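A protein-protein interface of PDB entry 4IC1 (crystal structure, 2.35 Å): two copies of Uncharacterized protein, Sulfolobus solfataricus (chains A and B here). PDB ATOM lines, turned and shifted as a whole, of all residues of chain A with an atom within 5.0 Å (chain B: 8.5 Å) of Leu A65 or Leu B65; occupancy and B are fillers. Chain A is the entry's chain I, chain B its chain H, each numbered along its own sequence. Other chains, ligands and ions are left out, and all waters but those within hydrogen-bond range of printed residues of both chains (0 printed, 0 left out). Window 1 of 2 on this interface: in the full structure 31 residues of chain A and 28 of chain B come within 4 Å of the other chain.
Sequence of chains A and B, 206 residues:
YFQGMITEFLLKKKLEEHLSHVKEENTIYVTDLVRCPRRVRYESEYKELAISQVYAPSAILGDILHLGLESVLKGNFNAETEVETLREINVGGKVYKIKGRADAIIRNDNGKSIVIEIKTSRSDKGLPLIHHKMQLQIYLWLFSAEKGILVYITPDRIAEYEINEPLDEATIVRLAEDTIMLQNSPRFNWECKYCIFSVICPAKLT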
ATOM      1  N   ILE A  60      30.749 -31.254 -10.656  1.00  0.00           N
ATOM      2  CA  ILE A  60      29.909 -30.614 -11.649  1.00  0.00           C
ATOM      3  C   ILE A  60      28.992 -29.593 -10.968  1.00  0.00           C
ATOM      4  O   ILE A  60      28.889 -28.434 -11.383  1.00  0.00           O
ATOM      5  CB  ILE A  60      29.028 -31.630 -12.419  1.00  0.00           C
ATOM      6  CG1 ILE A  60      29.851 -32.476 -13.409  1.00  0.00           C
ATOM      7  CG2 ILE A  60      27.964 -30.893 -13.192  1.00  0.00           C
ATOM      8  CD1 ILE A  60      29.090 -33.698 -13.974  1.00  0.00           C
ATOM      9  N   LEU A  61      28.326 -30.043  -9.915  1.00  0.00           N
ATOM     10  CA  LEU A  61      27.440 -29.192  -9.169  1.00  0.00           C
ATOM     11  C   LEU A  61      28.193 -27.990  -8.622  1.00  0.00           C
ATOM     12  O   LEU A  61      27.703 -26.893  -8.717  1.00  0.00           O
ATOM     13  CB  LEU A  61      26.776 -29.982  -8.066  1.00  0.00           C
ATOM     14  CG  LEU A  61      25.716 -29.253  -7.269  1.00  0.00           C
ATOM     15  CD1 LEU A  61      24.822 -30.259  -6.657  1.00  0.00           C
ATOM     16  CD2 LEU A  61      26.402 -28.425  -6.219  1.00  0.00           C
ATOM     17  N   GLY A  62      29.392 -28.199  -8.099  1.00  0.00           N
ATOM     18  CA  GLY A  62      30.220 -27.103  -7.590  1.00  0.00           C
ATOM     19  C   GLY A  62      30.585 -26.109  -8.672  1.00  0.00           C
ATOM     20  O   GLY A  62      30.566 -24.891  -8.465  1.00  0.00           O
ATOM     21  N   ASP A  63      30.904 -26.620  -9.853  1.00  0.00           N
ATOM     22  CA  ASP A  63      31.238 -25.741 -10.935  1.00  0.00           C
ATOM     23  C   ASP A  63      30.041 -24.897 -11.231  1.00  0.00           C
ATOM     24  O   ASP A  63      30.175 -23.689 -11.238  1.00  0.00           O
ATOM     25  CB  ASP A  63      31.647 -26.514 -12.175  1.00  0.00           C
ATOM     26  CG  ASP A  63      33.025 -27.104 -12.061  1.00  0.00           C
ATOM     27  OD1 ASP A  63      33.920 -26.421 -11.498  1.00  0.00           O
ATOM     28  OD2 ASP A  63      33.204 -28.253 -12.546  1.00  0.00           O
ATOM     29  N   ILE A  64      28.889 -25.531 -11.472  1.00  0.00           N
ATOM     30  CA  ILE A  64      27.671 -24.848 -11.860  1.00  0.00           C
ATOM     31  C   ILE A  64      27.363 -23.751 -10.863  1.00  0.00           C
ATOM     32  O   ILE A  64      26.852 -22.677 -11.209  1.00  0.00           O
ATOM     33  CB  ILE A  64      26.493 -25.815 -11.962  1.00  0.00           C
ATOM     34  CG1 ILE A  64      26.690 -26.757 -13.150  1.00  0.00           C
ATOM     35  CG2 ILE A  64      25.173 -25.080 -12.153  1.00  0.00           C
ATOM     36  CD1 ILE A  64      25.521 -27.669 -13.439  1.00  0.00           C
ATOM     37  N   LEU A  65      27.725 -23.997  -9.617  1.00  0.00           N
ATOM     38  CA  LEU A  65      27.544 -23.006  -8.581  1.00  0.00           C
ATOM     39  C   LEU A  65      28.348 -21.752  -8.797  1.00  0.00           C
ATOM     40  O   LEU A  65      27.790 -20.670  -8.739  1.00  0.00           O
ATOM     41  CB  LEU A  65      27.935 -23.558  -7.215  1.00  0.00           C
ATOM     42  CG  LEU A  65      27.468 -22.658  -6.070  1.00  0.00           C
ATOM     43  CD1 LEU A  65      25.966 -22.961  -5.728  1.00  0.00           C
ATOM     44  CD2 LEU A  65      28.401 -22.832  -4.884  1.00  0.00           C
ATOM     45  N   HIS A  66      29.661 -21.907  -8.982  1.00  0.00           N
ATOM     46  CA  HIS A  66      30.544 -20.770  -9.144  1.00  0.00           C
ATOM     47  C   HIS A  66      30.061 -19.974 -10.354  1.00  0.00           C
ATOM     48  O   HIS A  66      29.965 -18.741 -10.315  1.00  0.00           O
ATOM     49  CB  HIS A  66      31.991 -21.230  -9.310  1.00  0.00           C
ATOM     50  CG  HIS A  66      32.583 -21.875  -8.086  1.00  0.00           C
ATOM     51  ND1 HIS A  66      32.305 -23.174  -7.710  1.00  0.00           N
ATOM     52  CD2 HIS A  66      33.466 -21.403  -7.179  1.00  0.00           C
ATOM     53  CE1 HIS A  66      32.996 -23.473  -6.622  1.00  0.00           C
ATOM     54  NE2 HIS A  66      33.713 -22.416  -6.279  1.00  0.00           N
ATOM     55  N   LEU A  67      29.665 -20.680 -11.397  1.00  0.00           N
ATOM     56  CA  LEU A  67      29.103 -20.039 -12.570  1.00  0.00           C
ATOM     57  C   LEU A  67      27.961 -19.108 -12.117  1.00  0.00           C
ATOM     58  O   LEU A  67      27.980 -17.895 -12.352  1.00  0.00           O
ATOM     59  CB  LEU A  67      28.587 -21.101 -13.541  1.00  0.00           C
ATOM     60  CG  LEU A  67      28.894 -21.105 -15.058  1.00  0.00           C
ATOM     61  CD1 LEU A  67      29.483 -22.464 -15.526  1.00  0.00           C
ATOM     62  CD2 LEU A  67      27.627 -20.814 -15.858  1.00  0.00           C
ATOM     63  N   GLY A  68      26.973 -19.667 -11.428  1.00  0.00           N
ATOM     64  CA  GLY A  68      25.811 -18.872 -11.037  1.00  0.00           C
ATOM     65  C   GLY A  68      26.135 -17.704 -10.112  1.00  0.00           C
ATOM     66  O   GLY A  68      25.421 -16.730 -10.060  1.00  0.00           O
ATOM     67  N   LEU A  69      27.220 -17.808  -9.370  1.00  0.00           N
ATOM     68  CA  LEU A  69      27.452 -16.907  -8.275  1.00  0.00           C
ATOM     69  C   LEU A  69      28.254 -15.748  -8.777  1.00  0.00           C
ATOM     70  O   LEU A  69      28.356 -14.711  -8.129  1.00  0.00           O
ATOM     71  CB  LEU A  69      28.227 -17.641  -7.189  1.00  0.00           C
ATOM     72  CG  LEU A  69      28.072 -17.208  -5.737  1.00  0.00           C
ATOM     73  CD1 LEU A  69      26.634 -17.284  -5.317  1.00  0.00           C
ATOM     74  CD2 LEU A  69      28.950 -18.083  -4.897  1.00  0.00           C
ATOM     75  N   ILE A 118      34.707 -20.068  -2.541  1.00  0.00           N
ATOM     76  CA  ILE A 118      33.339 -20.534  -2.389  1.00  0.00           C
ATOM     77  C   ILE A 118      33.303 -22.055  -2.293  1.00  0.00           C
ATOM     78  O   ILE A 118      33.907 -22.750  -3.112  1.00  0.00           O
ATOM     79  CB  ILE A 118      32.525 -20.105  -3.606  1.00  0.00           C
ATOM     80  CG1 ILE A 118      32.313 -18.583  -3.572  1.00  0.00           C
ATOM     81  CG2 ILE A 118      31.177 -20.861  -3.704  1.00  0.00           C
ATOM     82  CD1 ILE A 118      32.197 -17.999  -4.969  1.00  0.00           C
ATOM     83  N   LYS A 119      32.599 -22.596  -1.307  1.00  0.00           N
ATOM     84  CA  LYS A 119      32.514 -24.072  -1.191  1.00  0.00           C
ATOM     85  C   LYS A 119      31.088 -24.536  -1.125  1.00  0.00           C
ATOM     86  O   LYS A 119      30.231 -23.855  -0.545  1.00  0.00           O
ATOM     87  CB  LYS A 119      33.258 -24.566   0.045  1.00  0.00           C
ATOM     88  CG  LYS A 119      34.711 -24.224   0.045  1.00  0.00           C
ATOM     89  CD  LYS A 119      35.481 -25.092  -0.931  1.00  0.00           C
ATOM     90  CE  LYS A 119      36.966 -24.744  -0.846  1.00  0.00           C
ATOM     91  NZ  LYS A 119      37.824 -25.290  -1.920  1.00  0.00           N
ATOM     92  N   THR A 120      30.845 -25.685  -1.746  1.00  0.00           N
ATOM     93  CA  THR A 120      29.649 -26.451  -1.506  1.00  0.00           C
ATOM     94  C   THR A 120      29.978 -27.761  -0.806  1.00  0.00           C
ATOM     95  O   THR A 120      30.898 -28.442  -1.149  1.00  0.00           O
ATOM     96  CB  THR A 120      28.957 -26.891  -2.775  1.00  0.00           C
ATOM     97  OG1 THR A 120      29.581 -26.307  -3.931  1.00  0.00           O
ATOM     98  CG2 THR A 120      27.459 -26.561  -2.659  1.00  0.00           C
ATOM     99  N   ILE A 153      28.120 -22.828   0.763  1.00  0.00           N
ATOM    100  CA  ILE A 153      26.696 -22.905   0.423  1.00  0.00           C
ATOM    101  C   ILE A 153      26.315 -24.374   0.545  1.00  0.00           C
ATOM    102  O   ILE A 153      26.627 -25.163  -0.352  1.00  0.00           O
ATOM    103  CB  ILE A 153      26.378 -22.408  -1.048  1.00  0.00           C
ATOM    104  CG1 ILE A 153      26.998 -21.042  -1.349  1.00  0.00           C
ATOM    105  CG2 ILE A 153      24.864 -22.308  -1.354  1.00  0.00           C
ATOM    106  CD1 ILE A 153      26.554 -19.963  -0.449  1.00  0.00           C
ATOM    107  N   LEU B  10      23.467 -11.734  -0.610  1.00  0.00           N
ATOM    108  CA  LEU B  10      22.645 -12.795  -1.160  1.00  0.00           C
ATOM    109  C   LEU B  10      21.270 -12.847  -0.506  1.00  0.00           C
ATOM    110  O   LEU B  10      20.258 -13.080  -1.185  1.00  0.00           O
ATOM    111  CB  LEU B  10      23.362 -14.130  -1.041  1.00  0.00           C
ATOM    112  CG  LEU B  10      24.672 -14.289  -1.821  1.00  0.00           C
ATOM    113  CD1 LEU B  10      25.214 -15.679  -1.628  1.00  0.00           C
ATOM    114  CD2 LEU B  10      24.442 -14.005  -3.314  1.00  0.00           C
ATOM    115  N   PRO B  57      18.348 -22.423   3.152  1.00  0.00           N
ATOM    116  CA  PRO B  57      19.618 -22.557   2.425  1.00  0.00           C
ATOM    117  C   PRO B  57      19.474 -23.460   1.210  1.00  0.00           C
ATOM    118  O   PRO B  57      20.154 -23.267   0.204  1.00  0.00           O
ATOM    119  CB  PRO B  57      20.554 -23.215   3.440  1.00  0.00           C
ATOM    120  CG  PRO B  57      19.791 -23.195   4.779  1.00  0.00           C
ATOM    121  CD  PRO B  57      18.359 -23.210   4.403  1.00  0.00           C
ATOM    122  N   SER B  58      18.575 -24.435   1.290  1.00  0.00           N
ATOM    123  CA  SER B  58      18.310 -25.186   0.098  1.00  0.00           C
ATOM    124  C   SER B  58      17.796 -24.335  -1.011  1.00  0.00           C
ATOM    125  O   SER B  58      18.150 -24.577  -2.117  1.00  0.00           O
ATOM    126  CB  SER B  58      17.358 -26.345   0.308  1.00  0.00           C
ATOM    127  OG  SER B  58      18.149 -27.406   0.808  1.00  0.00           O
ATOM    128  N   ALA B  59      16.893 -23.416  -0.737  1.00  0.00           N
ATOM    129  CA  ALA B  59      16.407 -22.562  -1.812  1.00  0.00           C
ATOM    130  C   ALA B  59      17.547 -21.658  -2.318  1.00  0.00           C
ATOM    131  O   ALA B  59      17.727 -21.522  -3.491  1.00  0.00           O
ATOM    132  CB  ALA B  59      15.173 -21.730  -1.358  1.00  0.00           C
ATOM    133  N   ILE B  60      18.351 -21.109  -1.435  1.00  0.00           N
ATOM    134  CA  ILE B  60      19.470 -20.290  -1.865  1.00  0.00           C
ATOM    135  C   ILE B  60      20.396 -21.055  -2.766  1.00  0.00           C
ATOM    136  O   ILE B  60      20.702 -20.617  -3.851  1.00  0.00           O
ATOM    137  CB  ILE B  60      20.242 -19.733  -0.673  1.00  0.00           C
ATOM    138  CG1 ILE B  60      19.327 -18.794   0.127  1.00  0.00           C
ATOM    139  CG2 ILE B  60      21.510 -19.069  -1.128  1.00  0.00           C
ATOM    140  CD1 ILE B  60      19.889 -18.377   1.463  1.00  0.00           C
ATOM    141  N   LEU B  61      20.860 -22.194  -2.320  1.00  0.00           N
ATOM    142  CA  LEU B  61      21.663 -23.111  -3.173  1.00  0.00           C
ATOM    143  C   LEU B  61      20.943 -23.382  -4.464  1.00  0.00           C
ATOM    144  O   LEU B  61      21.563 -23.471  -5.484  1.00  0.00           O
ATOM    145  CB  LEU B  61      21.911 -24.460  -2.480  1.00  0.00           C
ATOM    146  CG  LEU B  61      22.806 -25.541  -3.124  1.00  0.00           C
ATOM    147  CD1 LEU B  61      24.089 -24.912  -3.584  1.00  0.00           C
ATOM    148  CD2 LEU B  61      23.148 -26.745  -2.103  1.00  0.00           C
ATOM    149  N   GLY B  62      19.630 -23.525  -4.399  1.00  0.00           N
ATOM    150  CA  GLY B  62      18.807 -23.868  -5.553  1.00  0.00           C
ATOM    151  C   GLY B  62      18.745 -22.764  -6.593  1.00  0.00           C
ATOM    152  O   GLY B  62      18.841 -23.052  -7.788  1.00  0.00           O
ATOM    153  N   ASP B  63      18.580 -21.515  -6.146  1.00  0.00           N
ATOM    154  CA  ASP B  63      18.525 -20.356  -7.047  1.00  0.00           C
ATOM    155  C   ASP B  63      19.860 -20.144  -7.753  1.00  0.00           C
ATOM    156  O   ASP B  63      19.897 -19.924  -8.959  1.00  0.00           O
ATOM    157  CB  ASP B  63      18.204 -19.082  -6.273  1.00  0.00           C
ATOM    158  CG  ASP B  63      16.762 -19.016  -5.803  1.00  0.00           C
ATOM    159  OD1 ASP B  63      15.887 -19.629  -6.457  1.00  0.00           O
ATOM    160  OD2 ASP B  63      16.517 -18.349  -4.760  1.00  0.00           O
ATOM    161  N   ILE B  64      20.953 -20.229  -6.993  1.00  0.00           N
ATOM    162  CA  ILE B  64      22.255 -20.053  -7.546  1.00  0.00           C
ATOM    163  C   ILE B  64      22.494 -21.064  -8.624  1.00  0.00           C
ATOM    164  O   ILE B  64      22.974 -20.699  -9.712  1.00  0.00           O
ATOM    165  CB  ILE B  64      23.299 -20.172  -6.511  1.00  0.00           C
ATOM    166  CG1 ILE B  64      23.204 -18.999  -5.558  1.00  0.00           C
ATOM    167  CG2 ILE B  64      24.641 -20.177  -7.128  1.00  0.00           C
ATOM    168  CD1 ILE B  64      24.172 -19.080  -4.409  1.00  0.00           C
ATOM    169  N   LEU B  65      22.135 -22.322  -8.376  1.00  0.00           N
ATOM    170  CA  LEU B  65      22.362 -23.369  -9.379  1.00  0.00           C
ATOM    171  C   LEU B  65      21.472 -23.226 -10.578  1.00  0.00           C
ATOM    172  O   LEU B  65      21.825 -23.738 -11.625  1.00  0.00           O
ATOM    173  CB  LEU B  65      22.099 -24.766  -8.825  1.00  0.00           C
ATOM    174  CG  LEU B  65      23.168 -25.285  -7.896  1.00  0.00           C
ATOM    175  CD1 LEU B  65      22.585 -26.497  -7.161  1.00  0.00           C
ATOM    176  CD2 LEU B  65      24.541 -25.607  -8.657  1.00  0.00           C
ATOM    177  N   HIS B  66      20.284 -22.637 -10.418  1.00  0.00           N
ATOM    178  CA  HIS B  66      19.443 -22.328 -11.585  1.00  0.00           C
ATOM    179  C   HIS B  66      20.168 -21.257 -12.404  1.00  0.00           C
ATOM    180  O   HIS B  66      20.213 -21.331 -13.625  1.00  0.00           O
ATOM    181  CB  HIS B  66      18.021 -21.868 -11.217  1.00  0.00           C
ATOM    182  CG  HIS B  66      17.028 -22.987 -11.036  1.00  0.00           C
ATOM    183  ND1 HIS B  66      17.112 -23.914 -10.011  1.00  0.00           N
ATOM    184  CD2 HIS B  66      15.899 -23.306 -11.722  1.00  0.00           C
ATOM    185  CE1 HIS B  66      16.078 -24.743 -10.070  1.00  0.00           C
ATOM    186  NE2 HIS B  66      15.324 -24.397 -11.095  1.00  0.00           N
ATOM    187  N   LEU B  67      20.786 -20.295 -11.728  1.00  0.00           N
ATOM    188  CA  LEU B  67      21.452 -19.186 -12.422  1.00  0.00           C
ATOM    189  C   LEU B  67      22.598 -19.726 -13.300  1.00  0.00           C
ATOM    190  O   LEU B  67      22.691 -19.400 -14.493  1.00  0.00           O
ATOM    191  CB  LEU B  67      21.971 -18.117 -11.420  1.00  0.00           C
ATOM    192  CG  LEU B  67      21.413 -16.672 -11.449  1.00  0.00           C
ATOM    193  CD1 LEU B  67      19.852 -16.564 -11.471  1.00  0.00           C
ATOM    194  CD2 LEU B  67      22.003 -15.852 -10.290  1.00  0.00           C
ATOM    195  N   GLY B  68      23.447 -20.564 -12.705  1.00  0.00           N
ATOM    196  CA  GLY B  68      24.621 -21.078 -13.403  1.00  0.00           C
ATOM    197  C   GLY B  68      24.228 -21.956 -14.571  1.00  0.00           C
ATOM    198  O   GLY B  68      24.847 -21.934 -15.598  1.00  0.00           O
ATOM    199  N   LEU B  69      23.200 -22.756 -14.407  1.00  0.00           N
ATOM    200  CA  LEU B  69      22.901 -23.742 -15.416  1.00  0.00           C
ATOM    201  C   LEU B  69      22.228 -22.968 -16.509  1.00  0.00           C
ATOM    202  O   LEU B  69      22.415 -23.282 -17.683  1.00  0.00           O
ATOM    203  CB  LEU B  69      22.011 -24.885 -14.916  1.00  0.00           C
ATOM    204  CG  LEU B  69      21.622 -25.889 -16.031  1.00  0.00           C
ATOM    205  CD1 LEU B  69      22.861 -26.480 -16.688  1.00  0.00           C
ATOM    206  CD2 LEU B  69      20.664 -27.010 -15.590  1.00  0.00           C
ATOM    207  N   GLU B  70      21.447 -21.956 -16.121  1.00  0.00           N
ATOM    208  CA  GLU B  70      20.764 -21.087 -17.092  1.00  0.00           C
ATOM    209  C   GLU B  70      21.804 -20.386 -17.978  1.00  0.00           C
ATOM    210  O   GLU B  70      21.744 -20.474 -19.200  1.00  0.00           O
ATOM    211  CB  GLU B  70      19.790 -20.101 -16.396  1.00  0.00           C
ATOM    212  CG  GLU B  70      18.359 -20.688 -16.269  1.00  0.00           C
ATOM    213  CD  GLU B  70      17.414 -20.001 -15.244  1.00  0.00           C
ATOM    214  OE1 GLU B  70      17.735 -18.900 -14.696  1.00  0.00           O
ATOM    215  OE2 GLU B  70      16.321 -20.599 -15.008  1.00  0.00           O
ATOM    216  N   SER B  71      22.794 -19.768 -17.347  1.00  0.00           N
ATOM    217  CA  SER B  71      23.905 -19.158 -18.059  1.00  0.00           C
ATOM    218  C   SER B  71      24.487 -20.039 -19.178  1.00  0.00           C
ATOM    219  O   SER B  71      24.793 -19.559 -20.270  1.00  0.00           O
ATOM    220  CB  SER B  71      24.999 -18.789 -17.064  1.00  0.00           C
ATOM    221  OG  SER B  71      26.262 -18.961 -17.673  1.00  0.00           O
ATOM    222  N   VAL B  72      24.667 -21.323 -18.883  1.00  0.00           N
ATOM    223  CA  VAL B  72      25.129 -22.303 -19.861  1.00  0.00           C
ATOM    224  C   VAL B  72      24.071 -22.532 -20.898  1.00  0.00           C
ATOM    225  O   VAL B  72      24.365 -22.697 -22.061  1.00  0.00           O
ATOM    226  CB  VAL B  72      25.361 -23.671 -19.196  1.00  0.00           C
ATOM    227  CG1 VAL B  72      25.763 -24.749 -20.250  1.00  0.00           C
ATOM    228  CG2 VAL B  72      26.407 -23.550 -18.092  1.00  0.00           C
ATOM    229  N   LEU B  73      22.816 -22.608 -20.468  1.00  0.00           N
ATOM    230  CA  LEU B  73      21.728 -22.901 -21.418  1.00  0.00           C
ATOM    231  C   LEU B  73      21.523 -21.772 -22.448  1.00  0.00           C
ATOM    232  O   LEU B  73      21.144 -22.047 -23.572  1.00  0.00           O
ATOM    233  CB  LEU B  73      20.407 -23.198 -20.705  1.00  0.00           C
ATOM    234  CG  LEU B  73      20.233 -24.527 -19.920  1.00  0.00           C
ATOM    235  CD1 LEU B  73      18.810 -24.671 -19.439  1.00  0.00           C
ATOM    236  CD2 LEU B  73      20.584 -25.774 -20.733  1.00  0.00           C
ATOM    237  N   ILE B 118      14.708 -27.336 -14.428  1.00  0.00           N
ATOM    238  CA  ILE B 118      15.901 -27.687 -13.699  1.00  0.00           C
ATOM    239  C   ILE B 118      15.516 -28.036 -12.228  1.00  0.00           C
ATOM    240  O   ILE B 118      14.695 -27.320 -11.641  1.00  0.00           O
ATOM    241  CB  ILE B 118      16.792 -26.504 -13.667  1.00  0.00           C
ATOM    242  CG1 ILE B 118      17.208 -26.145 -15.119  1.00  0.00           C
ATOM    243  CG2 ILE B 118      18.007 -26.766 -12.794  1.00  0.00           C
ATOM    244  CD1 ILE B 118      17.986 -24.900 -15.271  1.00  0.00           C
ATOM    245  N   LYS B 119      16.074 -29.125 -11.652  1.00  0.00           N
ATOM    246  CA  LYS B 119      15.876 -29.451 -10.211  1.00  0.00           C
ATOM    247  C   LYS B 119      17.163 -29.695  -9.491  1.00  0.00           C
ATOM    248  O   LYS B 119      18.108 -30.180 -10.060  1.00  0.00           O
ATOM    249  CB  LYS B 119      14.990 -30.649 -10.026  1.00  0.00           C
ATOM    250  CG  LYS B 119      13.598 -30.434 -10.503  1.00  0.00           C
ATOM    251  CD  LYS B 119      12.888 -29.293  -9.698  1.00  0.00           C
ATOM    252  CE  LYS B 119      11.458 -29.070 -10.223  1.00  0.00           C
ATOM    253  NZ  LYS B 119      10.754 -27.898  -9.577  1.00  0.00           N
ATOM    254  N   THR B 120      17.199 -29.333  -8.230  1.00  0.00           N
ATOM    255  CA  THR B 120      18.352 -29.614  -7.394  1.00  0.00           C
ATOM    256  C   THR B 120      17.799 -30.324  -6.167  1.00  0.00           C
ATOM    257  O   THR B 120      16.763 -29.958  -5.709  1.00  0.00           O
ATOM    258  CB  THR B 120      19.101 -28.310  -7.033  1.00  0.00           C
ATOM    259  OG1 THR B 120      18.185 -27.366  -6.461  1.00  0.00           O
ATOM    260  CG2 THR B 120      19.685 -27.700  -8.319  1.00  0.00           C
ATOM    261  N   SER B 121      18.433 -31.382  -5.719  1.00  0.00           N
ATOM    262  CA  SER B 121      17.983 -32.180  -4.591  1.00  0.00           C
ATOM    263  C   SER B 121      19.235 -32.606  -3.910  1.00  0.00           C
ATOM    264  O   SER B 121      20.298 -32.783  -4.538  1.00  0.00           O
ATOM    265  CB  SER B 121      17.309 -33.491  -4.987  1.00  0.00           C
ATOM    266  OG  SER B 121      16.067 -33.295  -5.636  1.00  0.00           O
ATOM    267  N   TYR B 152      18.151 -33.061 -13.300  1.00  0.00           N
ATOM    268  CA  TYR B 152      18.543 -32.983 -11.882  1.00  0.00           C
ATOM    269  C   TYR B 152      20.031 -32.725 -11.669  1.00  0.00           C
ATOM    270  O   TYR B 152      20.832 -33.341 -12.307  1.00  0.00           O
ATOM    271  CB  TYR B 152      18.192 -34.314 -11.207  1.00  0.00           C
ATOM    272  CG  TYR B 152      16.729 -34.494 -10.933  1.00  0.00           C
ATOM    273  CD1 TYR B 152      16.157 -34.009  -9.766  1.00  0.00           C
ATOM    274  CD2 TYR B 152      15.907 -35.157 -11.835  1.00  0.00           C
ATOM    275  CE1 TYR B 152      14.818 -34.195  -9.495  1.00  0.00           C
ATOM    276  CE2 TYR B 152      14.579 -35.352 -11.558  1.00  0.00           C
ATOM    277  CZ  TYR B 152      14.038 -34.839 -10.389  1.00  0.00           C
ATOM    278  OH  TYR B 152      12.688 -34.991 -10.145  1.00  0.00           O
ATOM    279  N   ILE B 153      20.397 -31.831 -10.766  1.00  0.00           N
ATOM    280  CA  ILE B 153      21.785 -31.695 -10.345  1.00  0.00           C
ATOM    281  C   ILE B 153      21.838 -32.010  -8.839  1.00  0.00           C
ATOM    282  O   ILE B 153      21.517 -31.168  -7.994  1.00  0.00           O
ATOM    283  CB  ILE B 153      22.340 -30.262 -10.530  1.00  0.00           C
ATOM    284  CG1 ILE B 153      22.137 -29.726 -11.963  1.00  0.00           C
ATOM    285  CG2 ILE B 153      23.800 -30.207 -10.156  1.00  0.00           C
ATOM    286  CD1 ILE B 153      22.710 -30.572 -13.054  1.00  0.00           C
ATOM    287  N   THR B 154      22.241 -33.227  -8.506  1.00  0.00           N
ATOM    288  CA  THR B 154      22.412 -33.656  -7.136  1.00  0.00           C
ATOM    289  C   THR B 154      23.883 -34.025  -6.906  1.00  0.00           C
ATOM    290  O   THR B 154      24.613 -34.321  -7.854  1.00  0.00           O
ATOM    291  CB  THR B 154      21.523 -34.866  -6.862  1.00  0.00           C
ATOM    292  OG1 THR B 154      22.227 -36.067  -7.181  1.00  0.00           O
ATOM    293  CG2 THR B 154      20.199 -34.791  -7.686  1.00  0.00           C
ATOM    294  N   PRO B 155      24.336 -34.032  -5.651  1.00  0.00           N
ATOM    295  CA  PRO B 155      25.719 -34.348  -5.299  1.00  0.00           C
ATOM    296  C   PRO B 155      26.139 -35.780  -5.561  1.00  0.00           C
ATOM    297  O   PRO B 155      27.317 -36.076  -5.492  1.00  0.00           O
ATOM    298  CB  PRO B 155      25.729 -34.128  -3.800  1.00  0.00           C
ATOM    299  CG  PRO B 155      24.613 -33.244  -3.533  1.00  0.00           C
ATOM    300  CD  PRO B 155      23.572 -33.621  -4.467  1.00  0.00           C
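N of Ile B153 sits at hydrogen-bond distance from O of Lys B119.
The backbone carbonyl oxygen (O) of Lys A119 is in hydrogen-bond range of the backbone NH (N) of Ile A153 (2.7 Å).
Of the 14 printed residues of chain A, 8 touch a printed residue of chain B.
Printed residues of chain A that touch a printed residue of chain B: Leu A61, Ile A64, Leu A65, Leu A67, Gly A68, Leu A69, Thr A120 and Ile A153.
Hydrophobic or aromatic side chains of chain A that line the printed part of chain B: Leu A61, Ile A64, Leu A65, Leu A67, Leu A69 and Ile A153.
Of the 26 printed residues of chain B, 11 touch a printed residue of chain A.
Among the printed residues, 19 pairs touch across the chains.
Among the printed residues, no Asp or Glu carboxylate lies within 4 Å of a Lys or Arg side-chain nitrogen of the other chain.
Leu A61 touches Leu B65, and with the chains exchanged Leu A65 touches Leu B61.
Leu A65 touches its own counterpart, Leu B65.
Gly A68 touches its own counterpart, Gly B68.
Thr A120 touches Leu B61, but with the chains exchanged Leu A61 does not touch Thr B120 (6.0 Å).
Of the 19 pairs that touch across the chains among the printed residues, 14 have their exchanged pair printed and touching as well.
Leu B65 touches Leu A61 (CD2 to O, 3.4 Å).
Leu A61 touches Ile B153.
Leu A61 touches Thr B154.
Leu B65 touches Ile A64.
Leu A65 touches Leu B61 (CD1 to CD1, 3.5 Å).
Val B72 touches Leu A67 (CG2 to CD2, 3.7 Å).
Ile B64 touches Gly A68.
Gly B68 touches Gly A68.
Leu A69 touches Ile B64 (CD1 to CD1, 3.2 Å).
Leu B61 touches Thr A120.
Of chain A, only Leu A61 (3.4 Å), Ile A64 (3.6 Å) and Leu A65 (3.7 Å) come within 4 Å of Leu B65.
Of the printed residues of chain A, Leu B61 touches Leu A65 (3.5 Å), Thr A120 (3.9 Å) and Ile A153 (3.5 Å).
Printed residues of chain A within 4 Å of Thr B154: Leu A61 (3.9 Å).
The nearest residue of chain B that does not touch Leu A65 is Gly B68 (5.7 Å).
The nearest printed residue of chain A that does not touch Leu B65 is Gly A62 (5.5 Å).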
